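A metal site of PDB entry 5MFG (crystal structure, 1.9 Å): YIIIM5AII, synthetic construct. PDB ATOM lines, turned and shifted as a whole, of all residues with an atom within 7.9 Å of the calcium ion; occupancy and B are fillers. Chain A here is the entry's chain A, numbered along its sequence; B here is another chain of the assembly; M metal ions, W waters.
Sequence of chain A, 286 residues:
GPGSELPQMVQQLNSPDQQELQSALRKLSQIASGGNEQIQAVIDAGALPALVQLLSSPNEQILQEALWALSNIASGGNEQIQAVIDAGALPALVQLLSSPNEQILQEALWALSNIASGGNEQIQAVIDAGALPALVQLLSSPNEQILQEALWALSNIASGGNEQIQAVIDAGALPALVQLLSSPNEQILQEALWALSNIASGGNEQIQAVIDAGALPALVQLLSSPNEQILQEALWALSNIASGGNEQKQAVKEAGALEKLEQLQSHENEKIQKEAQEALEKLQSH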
ATOM      1  N   SER A  57     -19.400 -24.067 -29.484  1.00  0.00           N
ATOM      2  CA  SER A  57     -18.604 -22.932 -29.036  1.00  0.00           C
ATOM      3  C   SER A  57     -17.727 -23.313 -27.839  1.00  0.00           C
ATOM      4  O   SER A  57     -18.203 -23.969 -26.912  1.00  0.00           O
ATOM      5  CB  SER A  57     -19.513 -21.761 -28.653  1.00  0.00           C
ATOM      6  OG  SER A  57     -18.781 -20.762 -27.966  1.00  0.00           O
ATOM      7  N   PRO A  58     -16.458 -22.918 -27.838  1.00  0.00           N
ATOM      8  CA  PRO A  58     -15.630 -23.073 -26.630  1.00  0.00           C
ATOM      9  C   PRO A  58     -15.868 -21.985 -25.595  1.00  0.00           C
ATOM     10  O   PRO A  58     -15.180 -21.985 -24.567  1.00  0.00           O
ATOM     11  CB  PRO A  58     -14.203 -22.993 -27.192  1.00  0.00           C
ATOM     12  CG  PRO A  58     -14.335 -22.080 -28.349  1.00  0.00           C
ATOM     13  CD  PRO A  58     -15.687 -22.335 -28.954  1.00  0.00           C
ATOM     14  N   ASN A  59     -16.801 -21.081 -25.843  1.00  0.00           N
ATOM     15  CA  ASN A  59     -17.149 -20.023 -24.899  1.00  0.00           C
ATOM     16  C   ASN A  59     -18.262 -20.543 -24.005  1.00  0.00           C
ATOM     17  O   ASN A  59     -19.420 -20.616 -24.422  1.00  0.00           O
ATOM     18  CB  ASN A  59     -17.554 -18.762 -25.639  1.00  0.00           C
ATOM     19  CG  ASN A  59     -17.897 -17.614 -24.712  1.00  0.00           C
ATOM     20  OD1 ASN A  59     -18.322 -17.825 -23.582  1.00  0.00           O
ATOM     21  ND2 ASN A  59     -17.704 -16.392 -25.189  1.00  0.00           N
ATOM     22  N   GLU A  60     -17.920 -20.900 -22.780  1.00  0.00           N
ATOM     23  CA  GLU A  60     -18.898 -21.495 -21.873  1.00  0.00           C
ATOM     24  C   GLU A  60     -20.031 -20.528 -21.574  1.00  0.00           C
ATOM     25  O   GLU A  60     -21.176 -20.951 -21.374  1.00  0.00           O
ATOM     26  CB  GLU A  60     -18.216 -21.933 -20.585  1.00  0.00           C
ATOM     27  CG  GLU A  60     -17.233 -23.087 -20.759  1.00  0.00           C
ATOM     28  CD  GLU A  60     -15.893 -22.662 -21.314  1.00  0.00           C
ATOM     29  OE1 GLU A  60     -15.735 -21.483 -21.680  1.00  0.00           O
ATOM     30  OE2 GLU A  60     -14.981 -23.512 -21.386  1.00  0.00           O
ATOM     31  N   GLN A  61     -19.751 -19.226 -21.545  1.00  0.00           N
ATOM     32  CA  GLN A  61     -20.795 -18.241 -21.285  1.00  0.00           C
ATOM     33  C   GLN A  61     -21.838 -18.248 -22.389  1.00  0.00           C
ATOM     34  O   GLN A  61     -23.038 -18.170 -22.117  1.00  0.00           O
ATOM     35  CB  GLN A  61     -20.161 -16.856 -21.140  1.00  0.00           C
ATOM     36  CG  GLN A  61     -21.147 -15.744 -20.853  1.00  0.00           C
ATOM     37  CD  GLN A  61     -20.465 -14.435 -20.526  1.00  0.00           C
ATOM     38  OE1 GLN A  61     -19.365 -14.152 -21.025  1.00  0.00           O
ATOM     39  NE2 GLN A  61     -21.086 -13.640 -19.674  1.00  0.00           N
ATOM     40  N   SER B 183      -9.128 -17.335 -15.826  1.00  0.00           N
ATOM     41  CA  SER B 183      -9.790 -18.544 -16.260  1.00  0.00           C
ATOM     42  C   SER B 183     -10.067 -18.482 -17.762  1.00  0.00           C
ATOM     43  O   SER B 183     -10.540 -17.445 -18.255  1.00  0.00           O
ATOM     44  CB  SER B 183     -11.098 -18.736 -15.497  1.00  0.00           C
ATOM     45  OG  SER B 183     -11.795 -19.889 -15.941  1.00  0.00           O
ATOM     46  N   PRO B 184      -9.797 -19.550 -18.519  1.00  0.00           N
ATOM     47  CA  PRO B 184     -10.263 -19.595 -19.911  1.00  0.00           C
ATOM     48  C   PRO B 184     -11.757 -19.841 -20.030  1.00  0.00           C
ATOM     49  O   PRO B 184     -12.249 -19.963 -21.164  1.00  0.00           O
ATOM     50  CB  PRO B 184      -9.464 -20.766 -20.491  1.00  0.00           C
ATOM     51  CG  PRO B 184      -9.233 -21.662 -19.341  1.00  0.00           C
ATOM     52  CD  PRO B 184      -9.038 -20.760 -18.159  1.00  0.00           C
ATOM     53  N   ASN B 185     -12.470 -19.933 -18.917  1.00  0.00           N
ATOM     54  CA  ASN B 185     -13.913 -20.140 -18.917  1.00  0.00           C
ATOM     55  C   ASN B 185     -14.578 -18.782 -18.754  1.00  0.00           C
ATOM     56  O   ASN B 185     -14.453 -18.134 -17.706  1.00  0.00           O
ATOM     57  CB  ASN B 185     -14.330 -21.082 -17.799  1.00  0.00           C
ATOM     58  CG  ASN B 185     -15.817 -21.330 -17.762  1.00  0.00           C
ATOM     59  OD1 ASN B 185     -16.617 -20.436 -18.031  1.00  0.00           O
ATOM     60  ND2 ASN B 185     -16.206 -22.554 -17.428  1.00  0.00           N
ATOM     61  N   GLU B 186     -15.310 -18.358 -19.791  1.00  0.00           N
ATOM     62  CA  GLU B 186     -15.943 -17.043 -19.771  1.00  0.00           C
ATOM     63  C   GLU B 186     -17.040 -16.956 -18.721  1.00  0.00           C
ATOM     64  O   GLU B 186     -17.229 -15.906 -18.095  1.00  0.00           O
ATOM     65  CB  GLU B 186     -16.497 -16.710 -21.157  1.00  0.00           C
ATOM     66  CG  GLU B 186     -15.435 -16.489 -22.236  1.00  0.00           C
ATOM     67  CD  GLU B 186     -14.886 -17.767 -22.834  1.00  0.00           C
ATOM     68  OE1 GLU B 186     -15.283 -18.869 -22.387  1.00  0.00           O
ATOM     69  OE2 GLU B 186     -14.045 -17.690 -23.753  1.00  0.00           O
ATOM     70  N   GLN B 187     -17.783 -18.042 -18.519  1.00  0.00           N
ATOM     71  CA  GLN B 187     -18.838 -18.029 -17.515  1.00  0.00           C
ATOM     72  C   GLN B 187     -18.256 -17.832 -16.125  1.00  0.00           C
ATOM     73  O   GLN B 187     -18.727 -16.992 -15.351  1.00  0.00           O
ATOM     74  CB  GLN B 187     -19.647 -19.327 -17.601  1.00  0.00           C
ATOM     75  CG  GLN B 187     -20.826 -19.386 -16.637  1.00  0.00           C
ATOM     76  CD  GLN B 187     -21.887 -18.353 -16.947  1.00  0.00           C
ATOM     77  OE1 GLN B 187     -22.134 -18.022 -18.098  1.00  0.00           O
ATOM     78  NE2 GLN B 187     -22.514 -17.825 -15.906  1.00  0.00           N
HETATM   79 CA    CA M   1     -13.847 -20.859 -22.911  1.00  0.00          CA
HETATM   80  O   HOH W   1     -13.170 -19.560 -25.209  1.00  0.00           O
HETATM   81  O   HOH W   2     -12.673 -22.875 -22.625  1.00  0.00           O
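The calcium ion is bound by OE1 of Glu 60, water W2, O of Pro 58, OE1 of Glu 186 of chain B, O of Pro 184 of chain B and water W1. The calcium ion has six donor atoms within binding distance.
OD1 of Asn 59 sits at hydrogen-bond distance from N of Gln 61 (2.9 Å). The backbone NH (N) of Asn 59 sits at hydrogen-bond distance from the side-chain hydroxyl (OG) of Ser 57 (2.9 Å). The side-chain carboxylate of Glu 186 of chain B sits close to the side-chain amide oxygen of Asn 59, 3.4 Å away.
Asn 59 touches the calcium ion. The nearest printed residue that does not touch the calcium ion is Asn 185 of chain B (4.1 Å).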
